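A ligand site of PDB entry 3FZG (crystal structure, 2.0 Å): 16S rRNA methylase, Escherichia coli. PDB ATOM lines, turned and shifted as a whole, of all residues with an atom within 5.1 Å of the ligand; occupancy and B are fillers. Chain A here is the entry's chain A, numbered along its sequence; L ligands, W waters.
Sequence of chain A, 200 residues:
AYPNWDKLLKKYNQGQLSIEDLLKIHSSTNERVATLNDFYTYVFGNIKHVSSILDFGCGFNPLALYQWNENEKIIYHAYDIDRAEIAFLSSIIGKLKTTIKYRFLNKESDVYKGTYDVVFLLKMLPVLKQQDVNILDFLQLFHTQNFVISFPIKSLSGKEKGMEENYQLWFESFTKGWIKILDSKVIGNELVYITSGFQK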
ATOM      1  N   HIS A  26     -28.010  -6.125   9.881  1.00  0.00           N
ATOM      2  CA  HIS A  26     -27.398  -7.338  10.414  1.00  0.00           C
ATOM      3  C   HIS A  26     -28.378  -8.012  11.378  1.00  0.00           C
ATOM      4  O   HIS A  26     -28.732  -7.433  12.410  1.00  0.00           O
ATOM      5  CB  HIS A  26     -26.077  -6.983  11.133  1.00  0.00           C
ATOM      6  CG  HIS A  26     -25.260  -8.177  11.504  1.00  0.00           C
ATOM      7  ND1 HIS A  26     -23.983  -8.380  11.011  1.00  0.00           N
ATOM      8  CD2 HIS A  26     -25.513  -9.217  12.326  1.00  0.00           C
ATOM      9  CE1 HIS A  26     -23.502  -9.503  11.514  1.00  0.00           C
ATOM     10  NE2 HIS A  26     -24.406 -10.037  12.314  1.00  0.00           N
ATOM     11  N   SER A  28     -28.151 -10.164  13.715  1.00  0.00           N
ATOM     12  CA  SER A  28     -27.788 -10.260  15.124  1.00  0.00           C
ATOM     13  C   SER A  28     -28.103  -8.959  15.869  1.00  0.00           C
ATOM     14  O   SER A  28     -28.492  -8.984  17.048  1.00  0.00           O
ATOM     15  CB  SER A  28     -26.307 -10.612  15.281  1.00  0.00           C
ATOM     16  OG  SER A  28     -26.064 -11.916  14.783  1.00  0.00           O
ATOM     17  N   THR A  29     -27.937  -7.823  15.205  1.00  0.00           N
ATOM     18  CA  THR A  29     -28.239  -6.548  15.846  1.00  0.00           C
ATOM     19  C   THR A  29     -29.745  -6.283  15.698  1.00  0.00           C
ATOM     20  O   THR A  29     -30.378  -5.726  16.601  1.00  0.00           O
ATOM     21  CB  THR A  29     -27.417  -5.388  15.244  1.00  0.00           C
ATOM     22  OG1 THR A  29     -26.078  -5.443  15.742  1.00  0.00           O
ATOM     23  CG2 THR A  29     -28.028  -4.036  15.611  1.00  0.00           C
ATOM     24  N   ARG A  32     -31.620  -7.634  18.456  1.00  0.00           N
ATOM     25  CA  ARG A  32     -31.383  -6.972  19.738  1.00  0.00           C
ATOM     26  C   ARG A  32     -32.057  -5.607  19.886  1.00  0.00           C
ATOM     27  O   ARG A  32     -32.233  -5.119  21.011  1.00  0.00           O
ATOM     28  CB  ARG A  32     -29.869  -6.843  19.948  1.00  0.00           C
ATOM     29  CG  ARG A  32     -29.439  -6.370  21.331  1.00  0.00           C
ATOM     30  CD  ARG A  32     -27.919  -6.457  21.490  1.00  0.00           C
ATOM     31  NE  ARG A  32     -27.434  -7.831  21.355  1.00  0.00           N
ATOM     32  CZ  ARG A  32     -26.725  -8.300  20.329  1.00  0.00           C
ATOM     33  NH1 ARG A  32     -26.396  -7.510  19.312  1.00  0.00           N
ATOM     34  NH2 ARG A  32     -26.352  -9.572  20.317  1.00  0.00           N
ATOM     35  N   ASP A  55     -15.139  -5.725  21.596  1.00  0.00           N
ATOM     36  CA  ASP A  55     -16.310  -6.401  21.028  1.00  0.00           C
ATOM     37  C   ASP A  55     -15.769  -7.311  19.924  1.00  0.00           C
ATOM     38  O   ASP A  55     -15.515  -6.861  18.801  1.00  0.00           O
ATOM     39  CB  ASP A  55     -17.265  -5.379  20.418  1.00  0.00           C
ATOM     40  CG  ASP A  55     -18.685  -5.911  20.286  1.00  0.00           C
ATOM     41  OD1 ASP A  55     -18.860  -7.158  20.362  1.00  0.00           O
ATOM     42  OD2 ASP A  55     -19.620  -5.103  20.101  1.00  0.00           O
ATOM     43  N   PHE A  56     -15.575  -8.592  20.251  1.00  0.00           N
ATOM     44  CA  PHE A  56     -15.027  -9.556  19.294  1.00  0.00           C
ATOM     45  C   PHE A  56     -16.126 -10.122  18.393  1.00  0.00           C
ATOM     46  O   PHE A  56     -17.088 -10.719  18.889  1.00  0.00           O
ATOM     47  CB  PHE A  56     -14.348 -10.712  20.052  1.00  0.00           C
ATOM     48  CG  PHE A  56     -13.542 -11.622  19.173  1.00  0.00           C
ATOM     49  CD1 PHE A  56     -12.167 -11.424  19.015  1.00  0.00           C
ATOM     50  CD2 PHE A  56     -14.161 -12.650  18.460  1.00  0.00           C
ATOM     51  CE1 PHE A  56     -11.425 -12.231  18.168  1.00  0.00           C
ATOM     52  CE2 PHE A  56     -13.416 -13.474  17.611  1.00  0.00           C
ATOM     53  CZ  PHE A  56     -12.048 -13.266  17.461  1.00  0.00           C
ATOM     54  N   GLY A  57     -15.974  -9.958  17.080  1.00  0.00           N
ATOM     55  CA  GLY A  57     -16.998 -10.414  16.148  1.00  0.00           C
ATOM     56  C   GLY A  57     -18.179  -9.468  16.356  1.00  0.00           C
ATOM     57  O   GLY A  57     -19.344  -9.881  16.393  1.00  0.00           O
ATOM     58  N   CYS A  58     -17.854  -8.187  16.468  1.00  0.00           N
ATOM     59  CA  CYS A  58     -18.822  -7.121  16.747  1.00  0.00           C
ATOM     60  C   CYS A  58     -20.050  -6.962  15.865  1.00  0.00           C
ATOM     61  O   CYS A  58     -21.095  -6.558  16.366  1.00  0.00           O
ATOM     62  CB  CYS A  58     -18.088  -5.776  16.811  1.00  0.00           C
ATOM     63  SG  CYS A  58     -17.428  -5.178  15.243  1.00  0.00           S
ATOM     64  N   GLY A  59     -19.937  -7.249  14.576  1.00  0.00           N
ATOM     65  CA  GLY A  59     -21.078  -7.076  13.695  1.00  0.00           C
ATOM     66  C   GLY A  59     -21.479  -5.601  13.699  1.00  0.00           C
ATOM     67  O   GLY A  59     -20.605  -4.735  13.634  1.00  0.00           O
ATOM     68  N   ASN A  61     -22.997  -4.113  16.196  1.00  0.00           N
ATOM     69  CA  ASN A  61     -23.140  -3.624  17.572  1.00  0.00           C
ATOM     70  C   ASN A  61     -22.482  -2.251  17.786  1.00  0.00           C
ATOM     71  O   ASN A  61     -22.951  -1.474  18.604  1.00  0.00           O
ATOM     72  CB  ASN A  61     -22.551  -4.626  18.570  1.00  0.00           C
ATOM     73  CG  ASN A  61     -22.971  -4.318  20.004  1.00  0.00           C
ATOM     74  OD1 ASN A  61     -22.186  -4.456  20.947  1.00  0.00           O
ATOM     75  ND2 ASN A  61     -24.221  -3.919  20.168  1.00  0.00           N
ATOM     76  N   TYR A  79     -13.835  -5.400  16.620  1.00  0.00           N
ATOM     77  CA  TYR A  79     -13.155  -6.301  15.698  1.00  0.00           C
ATOM     78  C   TYR A  79     -14.119  -7.327  15.088  1.00  0.00           C
ATOM     79  O   TYR A  79     -14.936  -7.916  15.789  1.00  0.00           O
ATOM     80  CB  TYR A  79     -12.037  -7.078  16.395  1.00  0.00           C
ATOM     81  CG  TYR A  79     -11.445  -8.152  15.519  1.00  0.00           C
ATOM     82  CD1 TYR A  79     -10.672  -7.821  14.402  1.00  0.00           C
ATOM     83  CD2 TYR A  79     -11.680  -9.504  15.784  1.00  0.00           C
ATOM     84  CE1 TYR A  79     -10.162  -8.802  13.567  1.00  0.00           C
ATOM     85  CE2 TYR A  79     -11.154 -10.499  14.942  1.00  0.00           C
ATOM     86  CZ  TYR A  79     -10.400 -10.137  13.834  1.00  0.00           C
ATOM     87  OH  TYR A  79      -9.901 -11.096  12.999  1.00  0.00           O
ATOM     88  N   ASP A  80     -14.031  -7.515  13.780  1.00  0.00           N
ATOM     89  CA  ASP A  80     -14.855  -8.492  13.094  1.00  0.00           C
ATOM     90  C   ASP A  80     -14.054  -8.964  11.891  1.00  0.00           C
ATOM     91  O   ASP A  80     -13.305  -8.198  11.286  1.00  0.00           O
ATOM     92  CB  ASP A  80     -16.200  -7.898  12.658  1.00  0.00           C
ATOM     93  CG  ASP A  80     -17.234  -8.964  12.305  1.00  0.00           C
ATOM     94  OD1 ASP A  80     -17.056  -9.654  11.286  1.00  0.00           O
ATOM     95  OD2 ASP A  80     -18.216  -9.121  13.063  1.00  0.00           O
ATOM     96  N   ILE A  81     -14.198 -10.244  11.550  1.00  0.00           N
ATOM     97  CA  ILE A  81     -13.463 -10.816  10.439  1.00  0.00           C
ATOM     98  C   ILE A  81     -13.853 -10.174   9.102  1.00  0.00           C
ATOM     99  O   ILE A  81     -13.072 -10.166   8.161  1.00  0.00           O
ATOM    100  CB  ILE A  81     -13.676 -12.344  10.370  1.00  0.00           C
ATOM    101  CG1 ILE A  81     -12.591 -12.987   9.499  1.00  0.00           C
ATOM    102  CG2 ILE A  81     -15.073 -12.665   9.831  1.00  0.00           C
ATOM    103  CD1 ILE A  81     -12.563 -14.492   9.587  1.00  0.00           C
ATOM    104  N   ASP A  82     -15.065  -9.615   9.037  1.00  0.00           N
ATOM    105  CA  ASP A  82     -15.521  -8.958   7.819  1.00  0.00           C
ATOM    106  C   ASP A  82     -14.920  -7.555   7.745  1.00  0.00           C
ATOM    107  O   ASP A  82     -15.477  -6.605   8.314  1.00  0.00           O
ATOM    108  CB  ASP A  82     -17.045  -8.889   7.788  1.00  0.00           C
ATOM    109  CG  ASP A  82     -17.578  -8.382   6.460  1.00  0.00           C
ATOM    110  OD1 ASP A  82     -16.898  -7.567   5.803  1.00  0.00           O
ATOM    111  OD2 ASP A  82     -18.687  -8.807   6.074  1.00  0.00           O
ATOM    112  N   GLU A  85     -17.130  -4.682   6.221  1.00  0.00           N
ATOM    113  CA  GLU A  85     -18.171  -4.264   7.144  1.00  0.00           C
ATOM    114  C   GLU A  85     -17.590  -3.288   8.163  1.00  0.00           C
ATOM    115  O   GLU A  85     -18.222  -2.298   8.522  1.00  0.00           O
ATOM    116  CB  GLU A  85     -18.754  -5.479   7.866  1.00  0.00           C
ATOM    117  CG  GLU A  85     -19.878  -5.139   8.838  1.00  0.00           C
ATOM    118  CD  GLU A  85     -20.572  -6.380   9.360  1.00  0.00           C
ATOM    119  OE1 GLU A  85     -19.909  -7.180  10.042  1.00  0.00           O
ATOM    120  OE2 GLU A  85     -21.769  -6.560   9.069  1.00  0.00           O
ATOM    121  N   LEU A 122     -20.869 -11.728  21.860  1.00  0.00           N
ATOM    122  CA  LEU A 122     -22.306 -11.822  21.652  1.00  0.00           C
ATOM    123  C   LEU A 122     -22.650 -12.720  20.467  1.00  0.00           C
ATOM    124  O   LEU A 122     -22.285 -12.428  19.336  1.00  0.00           O
ATOM    125  CB  LEU A 122     -22.878 -10.408  21.428  1.00  0.00           C
ATOM    126  CG  LEU A 122     -22.358  -9.328  22.384  1.00  0.00           C
ATOM    127  CD1 LEU A 122     -23.061  -8.000  22.114  1.00  0.00           C
ATOM    128  CD2 LEU A 122     -22.580  -9.762  23.819  1.00  0.00           C
ATOM    129  N   LYS A 123     -23.374 -13.805  20.751  1.00  0.00           N
ATOM    130  CA  LYS A 123     -23.772 -14.743  19.715  1.00  0.00           C
ATOM    131  C   LYS A 123     -22.531 -15.140  18.909  1.00  0.00           C
ATOM    132  O   LYS A 123     -22.568 -15.177  17.686  1.00  0.00           O
ATOM    133  CB  LYS A 123     -24.810 -14.089  18.795  1.00  0.00           C
ATOM    134  CG  LYS A 123     -26.048 -13.576  19.533  1.00  0.00           C
ATOM    135  CD  LYS A 123     -26.953 -12.732  18.632  1.00  0.00           C
ATOM    136  CE  LYS A 123     -28.164 -12.201  19.402  1.00  0.00           C
ATOM    137  NZ  LYS A 123     -28.971 -11.290  18.550  1.00  0.00           N
ATOM    138  N   MET A 124     -21.443 -15.435  19.624  1.00  0.00           N
ATOM    139  CA  MET A 124     -20.172 -15.793  19.000  1.00  0.00           C
ATOM    140  C   MET A 124     -19.671 -17.207  19.237  1.00  0.00           C
ATOM    141  O   MET A 124     -19.107 -17.828  18.335  1.00  0.00           O
ATOM    142  CB  MET A 124     -19.056 -14.826  19.444  1.00  0.00           C
ATOM    143  CG  MET A 124     -19.074 -13.478  18.780  1.00  0.00           C
ATOM    144  SD  MET A 124     -18.996 -13.580  16.991  1.00  0.00           S
ATOM    145  CE  MET A 124     -17.509 -14.543  16.742  1.00  0.00           C
ATOM    146  N   VAL A 127     -20.633 -19.817  16.626  1.00  0.00           N
ATOM    147  CA  VAL A 127     -19.936 -19.556  15.376  1.00  0.00           C
ATOM    148  C   VAL A 127     -18.491 -20.066  15.431  1.00  0.00           C
ATOM    149  O   VAL A 127     -18.030 -20.754  14.516  1.00  0.00           O
ATOM    150  CB  VAL A 127     -19.914 -18.041  15.052  1.00  0.00           C
ATOM    151  CG1 VAL A 127     -19.130 -17.794  13.784  1.00  0.00           C
ATOM    152  CG2 VAL A 127     -21.346 -17.530  14.912  1.00  0.00           C
ATOM    153  N   LEU A 128     -17.786 -19.720  16.504  1.00  0.00           N
ATOM    154  CA  LEU A 128     -16.398 -20.140  16.656  1.00  0.00           C
ATOM    155  C   LEU A 128     -16.285 -21.659  16.820  1.00  0.00           C
ATOM    156  O   LEU A 128     -15.405 -22.293  16.212  1.00  0.00           O
ATOM    157  CB  LEU A 128     -15.770 -19.430  17.869  1.00  0.00           C
ATOM    158  CG  LEU A 128     -15.642 -17.909  17.710  1.00  0.00           C
ATOM    159  CD1 LEU A 128     -15.180 -17.291  19.015  1.00  0.00           C
ATOM    160  CD2 LEU A 128     -14.652 -17.601  16.583  1.00  0.00           C
ATOM    161  N   GLN A 131     -16.287 -23.328  13.735  1.00  0.00           N
ATOM    162  CA  GLN A 131     -15.037 -23.170  13.025  1.00  0.00           C
ATOM    163  C   GLN A 131     -13.938 -23.997  13.673  1.00  0.00           C
ATOM    164  O   GLN A 131     -12.761 -23.845  13.366  1.00  0.00           O
ATOM    165  CB  GLN A 131     -14.642 -21.693  12.989  1.00  0.00           C
ATOM    166  CG  GLN A 131     -15.442 -20.873  11.990  1.00  0.00           C
ATOM    167  CD  GLN A 131     -15.311 -19.376  12.197  1.00  0.00           C
ATOM    168  OE1 GLN A 131     -14.287 -18.893  12.668  1.00  0.00           O
ATOM    169  NE2 GLN A 131     -16.342 -18.628  11.817  1.00  0.00           N
ATOM    170  N   GLU A 190     -32.315 -13.409  23.416  1.00  0.00           N
ATOM    171  CA  GLU A 190     -30.907 -13.672  23.696  1.00  0.00           C
ATOM    172  C   GLU A 190     -30.613 -14.033  25.154  1.00  0.00           C
ATOM    173  O   GLU A 190     -31.066 -13.368  26.082  1.00  0.00           O
ATOM    174  CB  GLU A 190     -30.129 -12.418  23.269  1.00  0.00           C
ATOM    175  CG  GLU A 190     -28.648 -12.366  23.576  1.00  0.00           C
ATOM    176  CD  GLU A 190     -27.981 -11.138  22.949  1.00  0.00           C
ATOM    177  OE1 GLU A 190     -28.645 -10.087  22.811  1.00  0.00           O
ATOM    178  OE2 GLU A 190     -26.777 -11.225  22.600  1.00  0.00           O
HETATM  179  N1  LIG L   1     -21.674 -10.108  17.838  1.00  0.00           N
HETATM  180  C1  LIG L   1     -22.664  -9.543  16.891  1.00  0.00           C
HETATM  181  C2  LIG L   1     -24.021  -9.440  17.560  1.00  0.00           C
HETATM  182  O1  LIG L   1     -24.324 -10.219  18.438  1.00  0.00           O
HETATM  183  O2  LIG L   1     -24.824  -8.578  17.217  1.00  0.00           O
HETATM  184  C3  LIG L   1     -22.747 -10.405  15.618  1.00  0.00           C
HETATM  185  C4  LIG L   1     -22.913 -11.909  15.948  1.00  0.00           C
HETATM  186  S1  LIG L   1     -23.029 -12.868  14.386  1.00  0.00           S
HETATM  187  C5  LIG L   1     -24.027 -14.281  14.954  1.00  0.00           C
HETATM  188  C6  LIG L   1     -21.390 -13.574  14.114  1.00  0.00           C
HETATM  189  C7  LIG L   1     -20.373 -12.469  13.851  1.00  0.00           C
HETATM  190  O3  LIG L   1     -19.048 -12.979  14.032  1.00  0.00           O
HETATM  191  C8  LIG L   1     -20.474 -11.956  12.412  1.00  0.00           C
HETATM  192  O4  LIG L   1     -20.475 -10.525  12.422  1.00  0.00           O
HETATM  193  C9  LIG L   1     -19.221 -12.541  11.702  1.00  0.00           C
HETATM  194  O5  LIG L   1     -18.776 -11.674  10.644  1.00  0.00           O
HETATM  195  C10 LIG L   1     -18.225 -12.648  12.883  1.00  0.00           C
HETATM  196  N2  LIG L   1     -17.210 -13.691  12.760  1.00  0.00           N
HETATM  197  C11 LIG L   1     -17.335 -14.932  12.194  1.00  0.00           C
HETATM  198  N3  LIG L   1     -16.213 -15.582  12.303  1.00  0.00           N
HETATM  199  C12 LIG L   1     -15.304 -14.799  12.946  1.00  0.00           C
HETATM  200  C13 LIG L   1     -13.956 -14.947  13.357  1.00  0.00           C
HETATM  201  N4  LIG L   1     -13.271 -16.126  13.110  1.00  0.00           N
HETATM  202  N5  LIG L   1     -13.349 -13.917  14.000  1.00  0.00           N
HETATM  203  C14 LIG L   1     -13.995 -12.769  14.258  1.00  0.00           C
HETATM  204  N6  LIG L   1     -15.267 -12.592  13.900  1.00  0.00           N
HETATM  205  C15 LIG L   1     -15.946 -13.568  13.249  1.00  0.00           C
HETATM  206  O   HOH W   1     -18.417 -12.880   7.966  1.00  0.00           O
HETATM  207  O   HOH W   2     -19.458  -9.938  20.069  1.00  0.00           O
HETATM  208  O   HOH W   3     -10.905 -16.847  15.040  1.00  0.00           O
HETATM  209  O   HOH W   4     -21.271  -7.514  19.114  1.00  0.00           O
HETATM  210  O   HOH W   5     -24.507  -7.483  14.562  1.00  0.00           O
HETATM  211  O   HOH W   6     -20.985  -9.489   9.894  1.00  0.00           O
HETATM  212  O   HOH W   7     -10.569 -13.494  13.734  1.00  0.00           O
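O2 of the ligand is in salt-bridge range of NH1 of Arg 32. A nitrogen (N4) of the ligand is in hydrogen-bond range of the side-chain amide oxygen (OE1) of Gln 131 (3.0 Å). N1 of the ligand is in hydrogen-bond range of O of Leu 122. An oxygen (O5) of the ligand sits at hydrogen-bond distance from the side-chain carboxylate (OD1) of Asp 80. The backbone carbonyl oxygen of Gly 57 sits at hydrogen-bond distance from a nitrogen (N1) of the ligand. The backbone NH (N) of Ile 81 sits at hydrogen-bond distance from a nitrogen (N6) of the ligand, at 3.5 Å.
N of Tyr 79 is in hydrogen-bond range of O of Asp 55, at 3.1 Å. The side-chain carboxylate of Glu 190 lies within salt-bridge range of the guanidinium group of Arg 32. N of Asp 82 sits at hydrogen-bond distance from OD1 of Asp 80 (3.0 Å). The backbone NH (N) of Gly 57 is in hydrogen-bond range of the backbone carbonyl oxygen (O) of Tyr 79 (2.6 Å). OG1 of Thr 29 lies within hydrogen-bond range of N of Asn 61. OD2 of Asp 80 sits at hydrogen-bond distance from N of Gly 59 (3.0 Å). O of Ser 28 is in hydrogen-bond range of NZ of Lys 123 (2.8 Å). N of Cys 58 sits at hydrogen-bond distance from O of Tyr 79, at 3.0 Å.
A ring nitrogen (NE2) of His 26 lies close to a sulfur (S1) of the ligand, at 3.8 Å. A sulfur (S1) of the ligand lies close to the side-chain hydroxyl (OG) of Ser 28 (3.2 Å). An oxygen (O3) of the ligand sits close to the side-chain sulfur of Met 124. Thr 29 touches the ligand. Phe 56 touches the ligand. O of Cys 58 touches C1 of the ligand, 3.4 Å away. Gly 59 touches the ligand (CA to O4, 3.7 Å). Tyr 79 touches the ligand. Lys 123 touches the ligand. Val 127 touches the ligand (CG1 to C11, 3.7 Å). 16 residues have an atom within 4 Å of the ligand: His 26, Ser 28, Thr 29, Arg 32, Phe 56, Gly 57, Cys 58, Gly 59, Tyr 79, Asp 80, Ile 81, Leu 122, Lys 123, Met 124, Val 127 and Gln 131. The nearest printed residue that does not touch the ligand is Leu 128 (4.02 Å).
Water W6 lies within hydrogen-bond range of the side-chain carboxylate of Glu 85 (2.6 Å), an oxygen (O4) of the ligand (2.8 Å) and a ring nitrogen (ND1) of His 26 (3.4 Å). Water W7 lies within hydrogen-bond range of the side-chain hydroxyl of Tyr 79 (2.6 Å) and a nitrogen (N5) of the ligand (2.8 Å). Water W5 lies within hydrogen-bond range of OG1 of Thr 29 (2.8 Å), O2 of the ligand (2.9 Å) and NE2 of His 26 (3.4 Å). Water W4 lies within hydrogen-bond range of the side-chain carboxylate (OD1) of Asp 55 (2.7 Å), the backbone carbonyl oxygen (O) of Cys 58 (2.9 Å) and a nitrogen (N1) of the ligand (2.9 Å). Water W2 lies within hydrogen-bond range of O of Phe 56 (2.8 Å), OD1 of Asp 55 (2.9 Å), N of Leu 122 (2.9 Å) and N1 of the ligand (3.1 Å).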
